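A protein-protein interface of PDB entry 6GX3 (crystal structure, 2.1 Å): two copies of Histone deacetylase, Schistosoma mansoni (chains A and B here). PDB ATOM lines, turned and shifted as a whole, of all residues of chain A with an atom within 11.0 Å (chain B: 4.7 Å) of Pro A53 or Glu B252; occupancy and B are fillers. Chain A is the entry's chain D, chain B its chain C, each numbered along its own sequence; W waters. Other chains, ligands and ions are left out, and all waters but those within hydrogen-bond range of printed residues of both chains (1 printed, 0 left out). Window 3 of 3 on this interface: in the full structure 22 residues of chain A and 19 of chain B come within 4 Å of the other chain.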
ATOM      1  N   GLN A  49      19.563 -25.222 -20.811  1.00  0.00           N
ATOM      2  CA  GLN A  49      19.097 -24.758 -19.523  1.00  0.00           C
ATOM      3  C   GLN A  49      20.322 -24.297 -18.753  1.00  0.00           C
ATOM      4  O   GLN A  49      21.441 -24.615 -19.147  1.00  0.00           O
ATOM      5  CB  GLN A  49      18.316 -25.851 -18.802  1.00  0.00           C
ATOM      6  CG  GLN A  49      16.981 -26.121 -19.489  1.00  0.00           C
ATOM      7  CD  GLN A  49      16.172 -27.195 -18.818  1.00  0.00           C
ATOM      8  OE1 GLN A  49      16.405 -28.379 -19.027  1.00  0.00           O
ATOM      9  NE2 GLN A  49      15.207 -26.788 -18.010  1.00  0.00           N
ATOM     10  N   TRP A  50      20.112 -23.522 -17.691  1.00  0.00           N
ATOM     11  CA  TRP A  50      21.218 -22.874 -16.987  1.00  0.00           C
ATOM     12  C   TRP A  50      21.330 -23.301 -15.522  1.00  0.00           C
ATOM     13  O   TRP A  50      20.363 -23.773 -14.921  1.00  0.00           O
ATOM     14  CB  TRP A  50      21.073 -21.355 -17.057  1.00  0.00           C
ATOM     15  CG  TRP A  50      21.312 -20.772 -18.414  1.00  0.00           C
ATOM     16  CD1 TRP A  50      22.525 -20.527 -19.001  1.00  0.00           C
ATOM     17  CD2 TRP A  50      20.320 -20.340 -19.352  1.00  0.00           C
ATOM     18  NE1 TRP A  50      22.347 -19.969 -20.242  1.00  0.00           N
ATOM     19  CE2 TRP A  50      21.004 -19.839 -20.483  1.00  0.00           C
ATOM     20  CE3 TRP A  50      18.921 -20.328 -19.349  1.00  0.00           C
ATOM     21  CZ2 TRP A  50      20.337 -19.339 -21.603  1.00  0.00           C
ATOM     22  CZ3 TRP A  50      18.260 -19.812 -20.454  1.00  0.00           C
ATOM     23  CH2 TRP A  50      18.969 -19.326 -21.568  1.00  0.00           C
ATOM     24  N   ASP A  51      22.525 -23.119 -14.964  1.00  0.00           N
ATOM     25  CA  ASP A  51      22.846 -23.562 -13.617  1.00  0.00           C
ATOM     26  C   ASP A  51      22.297 -22.627 -12.555  1.00  0.00           C
ATOM     27  O   ASP A  51      22.211 -23.001 -11.382  1.00  0.00           O
ATOM     28  CB  ASP A  51      24.373 -23.683 -13.437  1.00  0.00           C
ATOM     29  CG  ASP A  51      25.000 -24.722 -14.363  1.00  0.00           C
ATOM     30  OD1 ASP A  51      24.235 -25.475 -15.011  1.00  0.00           O
ATOM     31  OD2 ASP A  51      26.255 -24.792 -14.428  1.00  0.00           O
ATOM     32  N   SER A  52      21.956 -21.404 -12.950  1.00  0.00           N
ATOM     33  CA  SER A  52      21.482 -20.414 -11.989  1.00  0.00           C
ATOM     34  C   SER A  52      20.827 -19.253 -12.696  1.00  0.00           C
ATOM     35  O   SER A  52      21.052 -19.067 -13.890  1.00  0.00           O
ATOM     36  CB  SER A  52      22.654 -19.899 -11.135  1.00  0.00           C
ATOM     37  OG  SER A  52      23.594 -19.207 -11.943  1.00  0.00           O
ATOM     38  N   PRO A  53      20.037 -18.450 -11.956  1.00  0.00           N
ATOM     39  CA  PRO A  53      19.582 -17.152 -12.470  1.00  0.00           C
ATOM     40  C   PRO A  53      20.712 -16.294 -13.043  1.00  0.00           C
ATOM     41  O   PRO A  53      20.522 -15.676 -14.083  1.00  0.00           O
ATOM     42  CB  PRO A  53      18.972 -16.478 -11.237  1.00  0.00           C
ATOM     43  CG  PRO A  53      18.511 -17.618 -10.375  1.00  0.00           C
ATOM     44  CD  PRO A  53      19.467 -18.756 -10.628  1.00  0.00           C
ATOM     45  N   SER A  54      21.866 -16.257 -12.376  1.00  0.00           N
ATOM     46  CA  SER A  54      22.983 -15.406 -12.809  1.00  0.00           C
ATOM     47  C   SER A  54      23.539 -15.808 -14.170  1.00  0.00           C
ATOM     48  O   SER A  54      23.854 -14.958 -15.013  1.00  0.00           O
ATOM     49  CB  SER A  54      24.103 -15.445 -11.767  1.00  0.00           C
ATOM     50  OG  SER A  54      23.649 -14.844 -10.566  1.00  0.00           O
ATOM     51  N   ARG A  55      23.665 -17.107 -14.388  1.00  0.00           N
ATOM     52  CA  ARG A  55      24.183 -17.581 -15.664  1.00  0.00           C
ATOM     53  C   ARG A  55      23.149 -17.345 -16.779  1.00  0.00           C
ATOM     54  O   ARG A  55      23.507 -17.007 -17.906  1.00  0.00           O
ATOM     55  CB  ARG A  55      24.576 -19.049 -15.561  1.00  0.00           C
ATOM     56  CG  ARG A  55      25.949 -19.252 -14.920  1.00  0.00           C
ATOM     57  CD  ARG A  55      26.322 -20.725 -14.839  1.00  0.00           C
ATOM     58  NE  ARG A  55      27.646 -20.931 -14.256  1.00  0.00           N
ATOM     59  CZ  ARG A  55      28.771 -20.938 -14.961  1.00  0.00           C
ATOM     60  NH1 ARG A  55      28.736 -20.747 -16.273  1.00  0.00           N
ATOM     61  NH2 ARG A  55      29.934 -21.136 -14.353  1.00  0.00           N
ATOM     62  N   MET A  56      21.867 -17.486 -16.465  1.00  0.00           N
ATOM     63  CA  MET A  56      20.851 -17.175 -17.463  1.00  0.00           C
ATOM     64  C   MET A  56      20.960 -15.694 -17.849  1.00  0.00           C
ATOM     65  O   MET A  56      21.065 -15.367 -19.031  1.00  0.00           O
ATOM     66  CB  MET A  56      19.447 -17.509 -16.955  1.00  0.00           C
ATOM     67  CG  MET A  56      18.350 -17.231 -17.971  1.00  0.00           C
ATOM     68  SD  MET A  56      17.701 -15.528 -17.882  1.00  0.00           S
ATOM     69  CE  MET A  56      16.781 -15.587 -16.343  1.00  0.00           C
ATOM     70  N   TYR A  57      20.974 -14.809 -16.851  1.00  0.00           N
ATOM     71  CA  TYR A  57      21.071 -13.379 -17.110  1.00  0.00           C
ATOM     72  C   TYR A  57      22.315 -13.030 -17.918  1.00  0.00           C
ATOM     73  O   TYR A  57      22.264 -12.177 -18.804  1.00  0.00           O
ATOM     74  CB  TYR A  57      21.066 -12.583 -15.794  1.00  0.00           C
ATOM     75  CG  TYR A  57      19.727 -11.960 -15.476  1.00  0.00           C
ATOM     76  CD1 TYR A  57      18.673 -12.742 -15.018  1.00  0.00           C
ATOM     77  CD2 TYR A  57      19.515 -10.593 -15.637  1.00  0.00           C
ATOM     78  CE1 TYR A  57      17.443 -12.184 -14.727  1.00  0.00           C
ATOM     79  CE2 TYR A  57      18.287 -10.019 -15.349  1.00  0.00           C
ATOM     80  CZ  TYR A  57      17.248 -10.823 -14.896  1.00  0.00           C
ATOM     81  OH  TYR A  57      16.009 -10.282 -14.605  1.00  0.00           O
ATOM     82  N   GLU A  58      23.422 -13.703 -17.618  1.00  0.00           N
ATOM     83  CA  GLU A  58      24.677 -13.460 -18.319  1.00  0.00           C
ATOM     84  C   GLU A  58      24.546 -13.849 -19.795  1.00  0.00           C
ATOM     85  O   GLU A  58      25.051 -13.166 -20.693  1.00  0.00           O
ATOM     86  CB  GLU A  58      25.819 -14.232 -17.647  1.00  0.00           C
ATOM     87  CG  GLU A  58      27.127 -14.279 -18.448  1.00  0.00           C
ATOM     88  CD  GLU A  58      28.259 -14.980 -17.696  1.00  0.00           C
ATOM     89  OE1 GLU A  58      28.273 -16.231 -17.644  1.00  0.00           O
ATOM     90  OE2 GLU A  58      29.130 -14.272 -17.147  1.00  0.00           O
ATOM     91  N   ALA A  59      23.860 -14.949 -20.042  1.00  0.00           N
ATOM     92  CA  ALA A  59      23.682 -15.414 -21.404  1.00  0.00           C
ATOM     93  C   ALA A  59      22.815 -14.421 -22.151  1.00  0.00           C
ATOM     94  O   ALA A  59      23.153 -14.003 -23.257  1.00  0.00           O
ATOM     95  CB  ALA A  59      23.057 -16.808 -21.434  1.00  0.00           C
ATOM     96  N   VAL A  60      21.704 -14.021 -21.541  1.00  0.00           N
ATOM     97  CA  VAL A  60      20.784 -13.146 -22.258  1.00  0.00           C
ATOM     98  C   VAL A  60      21.349 -11.723 -22.396  1.00  0.00           C
ATOM     99  O   VAL A  60      21.141 -11.070 -23.428  1.00  0.00           O
ATOM    100  CB  VAL A  60      19.406 -13.102 -21.588  1.00  0.00           C
ATOM    101  CG1 VAL A  60      18.470 -12.176 -22.360  1.00  0.00           C
ATOM    102  CG2 VAL A  60      18.820 -14.507 -21.516  1.00  0.00           C
ATOM    103  N   THR A  61      22.083 -11.242 -21.389  1.00  0.00           N
ATOM    104  CA  THR A  61      22.548  -9.855 -21.455  1.00  0.00           C
ATOM    105  C   THR A  61      23.852  -9.720 -22.228  1.00  0.00           C
ATOM    106  O   THR A  61      24.490  -8.677 -22.200  1.00  0.00           O
ATOM    107  CB  THR A  61      22.702  -9.215 -20.072  1.00  0.00           C
ATOM    108  OG1 THR A  61      23.595  -9.984 -19.260  1.00  0.00           O
ATOM    109  CG2 THR A  61      21.339  -9.116 -19.398  1.00  0.00           C
ATOM    110  N   ALA A  62      24.211 -10.777 -22.950  1.00  0.00           N
ATOM    111  CA  ALA A  62      25.271 -10.710 -23.951  1.00  0.00           C
ATOM    112  C   ALA A  62      24.820  -9.833 -25.124  1.00  0.00           C
ATOM    113  O   ALA A  62      25.636  -9.345 -25.905  1.00  0.00           O
ATOM    114  CB  ALA A  62      25.638 -12.104 -24.434  1.00  0.00           C
ATOM    115  N   THR A  66      20.387  -5.381 -19.143  1.00  0.00           N
ATOM    116  CA  THR A  66      19.853  -5.932 -17.905  1.00  0.00           C
ATOM    117  C   THR A  66      18.508  -5.321 -17.520  1.00  0.00           C
ATOM    118  O   THR A  66      17.615  -6.029 -17.061  1.00  0.00           O
ATOM    119  CB  THR A  66      20.821  -5.722 -16.731  1.00  0.00           C
ATOM    120  OG1 THR A  66      22.150  -6.076 -17.137  1.00  0.00           O
ATOM    121  CG2 THR A  66      20.390  -6.574 -15.525  1.00  0.00           C
ATOM    122  N   VAL A  69      15.804  -6.886 -19.600  1.00  0.00           N
ATOM    123  CA  VAL A  69      15.496  -8.245 -19.167  1.00  0.00           C
ATOM    124  C   VAL A  69      14.720  -8.197 -17.850  1.00  0.00           C
ATOM    125  O   VAL A  69      13.726  -8.919 -17.685  1.00  0.00           O
ATOM    126  CB  VAL A  69      16.760  -9.118 -19.036  1.00  0.00           C
ATOM    127  CG1 VAL A  69      16.418 -10.485 -18.427  1.00  0.00           C
ATOM    128  CG2 VAL A  69      17.379  -9.318 -20.421  1.00  0.00           C
ATOM    129  N   ASP A  70      15.132  -7.312 -16.947  1.00  0.00           N
ATOM    130  CA  ASP A  70      14.376  -7.052 -15.722  1.00  0.00           C
ATOM    131  C   ASP A  70      12.926  -6.658 -16.020  1.00  0.00           C
ATOM    132  O   ASP A  70      12.006  -7.199 -15.421  1.00  0.00           O
ATOM    133  CB  ASP A  70      15.042  -5.946 -14.898  1.00  0.00           C
ATOM    134  CG  ASP A  70      16.423  -6.342 -14.384  1.00  0.00           C
ATOM    135  OD1 ASP A  70      16.695  -7.558 -14.254  1.00  0.00           O
ATOM    136  OD2 ASP A  70      17.230  -5.428 -14.100  1.00  0.00           O
ATOM    137  N   LYS A  73      10.918  -9.648 -17.294  1.00  0.00           N
ATOM    138  CA  LYS A  73      10.553 -10.549 -16.208  1.00  0.00           C
ATOM    139  C   LYS A  73       9.506  -9.922 -15.281  1.00  0.00           C
ATOM    140  O   LYS A  73       8.638 -10.623 -14.750  1.00  0.00           O
ATOM    141  CB  LYS A  73      11.776 -10.967 -15.395  1.00  0.00           C
ATOM    142  CG  LYS A  73      11.613 -12.349 -14.805  1.00  0.00           C
ATOM    143  CD  LYS A  73      12.570 -12.608 -13.659  1.00  0.00           C
ATOM    144  CE  LYS A  73      12.429 -14.044 -13.163  1.00  0.00           C
ATOM    145  NZ  LYS A  73      11.007 -14.510 -13.193  1.00  0.00           N
ATOM    146  N   PHE A 109       7.893 -13.991 -20.567  1.00  0.00           N
ATOM    147  CA  PHE A 109       9.346 -14.138 -20.415  1.00  0.00           C
ATOM    148  C   PHE A 109       9.780 -15.591 -20.660  1.00  0.00           C
ATOM    149  O   PHE A 109      10.761 -15.830 -21.364  1.00  0.00           O
ATOM    150  CB  PHE A 109       9.825 -13.661 -19.030  1.00  0.00           C
ATOM    151  CG  PHE A 109      11.327 -13.643 -18.888  1.00  0.00           C
ATOM    152  CD1 PHE A 109      12.107 -12.882 -19.748  1.00  0.00           C
ATOM    153  CD2 PHE A 109      11.963 -14.392 -17.910  1.00  0.00           C
ATOM    154  CE1 PHE A 109      13.495 -12.869 -19.635  1.00  0.00           C
ATOM    155  CE2 PHE A 109      13.355 -14.380 -17.792  1.00  0.00           C
ATOM    156  CZ  PHE A 109      14.118 -13.622 -18.656  1.00  0.00           C
ATOM    157  N   LEU A 113      12.121 -16.689 -23.659  1.00  0.00           N
ATOM    158  CA  LEU A 113      13.376 -17.292 -23.230  1.00  0.00           C
ATOM    159  C   LEU A 113      13.527 -18.677 -23.859  1.00  0.00           C
ATOM    160  O   LEU A 113      14.634 -19.080 -24.228  1.00  0.00           O
ATOM    161  CB  LEU A 113      13.453 -17.365 -21.704  1.00  0.00           C
ATOM    162  CG  LEU A 113      14.806 -17.775 -21.106  1.00  0.00           C
ATOM    163  CD1 LEU A 113      15.908 -16.759 -21.402  1.00  0.00           C
ATOM    164  CD2 LEU A 113      14.655 -17.983 -19.622  1.00  0.00           C
ATOM    165  N   HIS B 211      14.789 -24.783  -5.893  1.00  0.00           N
ATOM    166  CA  HIS B 211      14.757 -23.557  -6.653  1.00  0.00           C
ATOM    167  C   HIS B 211      14.012 -23.744  -7.976  1.00  0.00           C
ATOM    168  O   HIS B 211      14.149 -24.770  -8.632  1.00  0.00           O
ATOM    169  CB  HIS B 211      16.145 -23.063  -6.952  1.00  0.00           C
ATOM    170  CG  HIS B 211      16.149 -21.779  -7.714  1.00  0.00           C
ATOM    171  ND1 HIS B 211      15.515 -20.646  -7.252  1.00  0.00           N
ATOM    172  CD2 HIS B 211      16.698 -21.449  -8.906  1.00  0.00           C
ATOM    173  CE1 HIS B 211      15.674 -19.668  -8.129  1.00  0.00           C
ATOM    174  NE2 HIS B 211      16.390 -20.127  -9.138  1.00  0.00           N
ATOM    175  N   SER B 213      13.111 -21.026 -11.424  1.00  0.00           N
ATOM    176  CA  SER B 213      13.189 -19.709 -12.040  1.00  0.00           C
ATOM    177  C   SER B 213      13.368 -19.924 -13.540  1.00  0.00           C
ATOM    178  O   SER B 213      13.804 -20.993 -13.943  1.00  0.00           O
ATOM    179  CB  SER B 213      14.350 -18.879 -11.452  1.00  0.00           C
ATOM    180  OG  SER B 213      15.613 -19.503 -11.627  1.00  0.00           O
ATOM    181  N   LEU B 250      11.304 -22.225  -4.337  1.00  0.00           N
ATOM    182  CA  LEU B 250      11.768 -21.095  -3.542  1.00  0.00           C
ATOM    183  C   LEU B 250      12.750 -20.222  -4.311  1.00  0.00           C
ATOM    184  O   LEU B 250      13.501 -20.704  -5.160  1.00  0.00           O
ATOM    185  CB  LEU B 250      12.423 -21.582  -2.249  1.00  0.00           C
ATOM    186  CG  LEU B 250      11.586 -22.462  -1.324  1.00  0.00           C
ATOM    187  CD1 LEU B 250      12.491 -23.038  -0.236  1.00  0.00           C
ATOM    188  CD2 LEU B 250      10.433 -21.659  -0.724  1.00  0.00           C
ATOM    189  N   GLU B 251      12.754 -18.934  -3.993  1.00  0.00           N
ATOM    190  CA  GLU B 251      13.653 -18.000  -4.641  1.00  0.00           C
ATOM    191  C   GLU B 251      15.096 -18.202  -4.156  1.00  0.00           C
ATOM    192  O   GLU B 251      15.340 -18.760  -3.081  1.00  0.00           O
ATOM    193  CB  GLU B 251      13.198 -16.561  -4.381  1.00  0.00           C
ATOM    194  CG  GLU B 251      11.733 -16.297  -4.698  1.00  0.00           C
ATOM    195  CD  GLU B 251      11.423 -16.295  -6.194  1.00  0.00           C
ATOM    196  OE1 GLU B 251      11.324 -17.391  -6.790  1.00  0.00           O
ATOM    197  OE2 GLU B 251      11.267 -15.198  -6.774  1.00  0.00           O
ATOM    198  N   GLU B 252      16.040 -17.738  -4.961  1.00  0.00           N
ATOM    199  CA  GLU B 252      17.457 -17.769  -4.612  1.00  0.00           C
ATOM    200  C   GLU B 252      17.775 -17.073  -3.285  1.00  0.00           C
ATOM    201  O   GLU B 252      17.149 -16.079  -2.931  1.00  0.00           O
ATOM    202  CB  GLU B 252      18.271 -17.119  -5.737  1.00  0.00           C
ATOM    203  CG  GLU B 252      19.763 -17.093  -5.477  1.00  0.00           C
ATOM    204  CD  GLU B 252      20.543 -16.402  -6.572  1.00  0.00           C
ATOM    205  OE1 GLU B 252      19.939 -16.066  -7.611  1.00  0.00           O
ATOM    206  OE2 GLU B 252      21.764 -16.198  -6.387  1.00  0.00           O
ATOM    207  N   GLY B 253      18.752 -17.598  -2.550  1.00  0.00           N
ATOM    208  CA  GLY B 253      19.353 -16.850  -1.463  1.00  0.00           C
ATOM    209  C   GLY B 253      18.946 -17.290  -0.071  1.00  0.00           C
ATOM    210  O   GLY B 253      19.462 -16.771   0.926  1.00  0.00           O
ATOM    211  N   ILE B 254      18.062 -18.280   0.001  1.00  0.00           N
ATOM    212  CA  ILE B 254      17.472 -18.681   1.268  1.00  0.00           C
ATOM    213  C   ILE B 254      18.478 -19.335   2.245  1.00  0.00           C
ATOM    214  O   ILE B 254      19.347 -20.113   1.835  1.00  0.00           O
ATOM    215  CB  ILE B 254      16.279 -19.626   1.015  1.00  0.00           C
ATOM    216  CG1 ILE B 254      15.358 -19.644   2.231  1.00  0.00           C
ATOM    217  CG2 ILE B 254      16.761 -21.032   0.646  1.00  0.00           C
ATOM    218  CD1 ILE B 254      14.048 -20.360   2.010  1.00  0.00           C
ATOM    219  N   ARG B 294      25.696 -22.049  -6.071  1.00  0.00           N
ATOM    220  CA  ARG B 294      25.617 -20.792  -5.314  1.00  0.00           C
ATOM    221  C   ARG B 294      24.213 -20.191  -5.289  1.00  0.00           C
ATOM    222  O   ARG B 294      24.070 -18.972  -5.299  1.00  0.00           O
ATOM    223  CB  ARG B 294      26.599 -19.756  -5.877  1.00  0.00           C
ATOM    224  CG  ARG B 294      28.083 -20.141  -5.775  1.00  0.00           C
ATOM    225  CD  ARG B 294      28.576 -20.056  -4.327  1.00  0.00           C
ATOM    226  NE  ARG B 294      28.179 -18.788  -3.713  1.00  0.00           N
ATOM    227  CZ  ARG B 294      28.468 -18.416  -2.469  1.00  0.00           C
ATOM    228  NH1 ARG B 294      29.176 -19.210  -1.670  1.00  0.00           N
ATOM    229  NH2 ARG B 294      28.048 -17.240  -2.022  1.00  0.00           N
ATOM    230  N   ILE B 295      23.185 -21.035  -5.226  1.00  0.00           N
ATOM    231  CA  ILE B 295      21.807 -20.534  -5.231  1.00  0.00           C
ATOM    232  C   ILE B 295      21.167 -20.455  -3.838  1.00  0.00           C
ATOM    233  O   ILE B 295      20.699 -19.387  -3.451  1.00  0.00           O
ATOM    234  CB  ILE B 295      20.911 -21.374  -6.149  1.00  0.00           C
ATOM    235  CG1 ILE B 295      21.329 -21.156  -7.602  1.00  0.00           C
ATOM    236  CG2 ILE B 295      19.464 -20.954  -6.010  1.00  0.00           C
ATOM    237  CD1 ILE B 295      20.873 -22.260  -8.519  1.00  0.00           C
ATOM    238  N   PHE B 296      21.125 -21.558  -3.090  1.00  0.00           N
ATOM    239  CA  PHE B 296      20.672 -21.479  -1.696  1.00  0.00           C
ATOM    240  C   PHE B 296      21.882 -21.262  -0.766  1.00  0.00           C
ATOM    241  O   PHE B 296      23.029 -21.274  -1.206  1.00  0.00           O
ATOM    242  CB  PHE B 296      19.890 -22.731  -1.262  1.00  0.00           C
ATOM    243  CG  PHE B 296      18.506 -22.848  -1.888  1.00  0.00           C
ATOM    244  CD1 PHE B 296      17.936 -21.782  -2.563  1.00  0.00           C
ATOM    245  CD2 PHE B 296      17.795 -24.042  -1.806  1.00  0.00           C
ATOM    246  CE1 PHE B 296      16.672 -21.901  -3.148  1.00  0.00           C
ATOM    247  CE2 PHE B 296      16.535 -24.170  -2.385  1.00  0.00           C
ATOM    248  CZ  PHE B 296      15.985 -23.113  -3.066  1.00  0.00           C
HETATM  249  O   HOH W   1      22.214 -16.740  -9.390  1.00  0.00           O
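No position is printed for both chains.
Of the 5 pairs that touch across the chains among the printed residues, none has its exchanged pair printed and touching as well.
A ring nitrogen (NE2) of His B211 sits at hydrogen-bond distance from the side-chain hydroxyl (OG) of Ser B213, at 2.7 Å.
ND1 of His B211 is in hydrogen-bond range of O of Leu B250.
N of Gly B253 is in hydrogen-bond range of O of Ile B295 (2.8 Å).
OG of Ser A52 sits close to N of Ser A54 (3.4 Å).
OG of Ser A52 is in hydrogen-bond range of N of Arg A55 (3.2 Å).
Hydrophobic or aromatic side chains of chain A within 4 Å of the printed part of chain B: Pro A53.
Of the 10 printed residues of chain B, 4 touch a printed residue of chain A.
Hydrophobic or aromatic side chains of chain B that line the printed part of chain A: His B211 and Ile B295.
Among the printed residues, 5 pairs touch across the chains.
Among the printed residues, no Asp or Glu carboxylate lies within 4 Å of a Lys or Arg side-chain nitrogen of the other chain.
Water W1 lies within hydrogen-bond range of the side-chain hydroxyl of Ser A54 (2.7 Å) and the side-chain carboxylate of Glu B252 (3.0 Å).
Of the printed residues of chain B, Asp A51 touches Ile B295 (3.2 Å).
Of chain B, only His B211 (3.5 Å), Ser B213 (3.7 Å) and Glu B252 (3.5 Å) come within 4 Å of Pro A53.
Of the printed residues of chain A, His B211 touches Pro A53.
Ser B213 touches just one residue of chain A: Pro A53.
Asp A51 touches Ile B295 (O to CD1, 3.2 Å).
Ser A52 touches Ile B295 (CB to CD1, 3.9 Å).
Pro A53 touches His B211.
CG of Pro A53 touches OG of Ser B213 (3.7 Å).
Pro A53 touches Glu B252.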
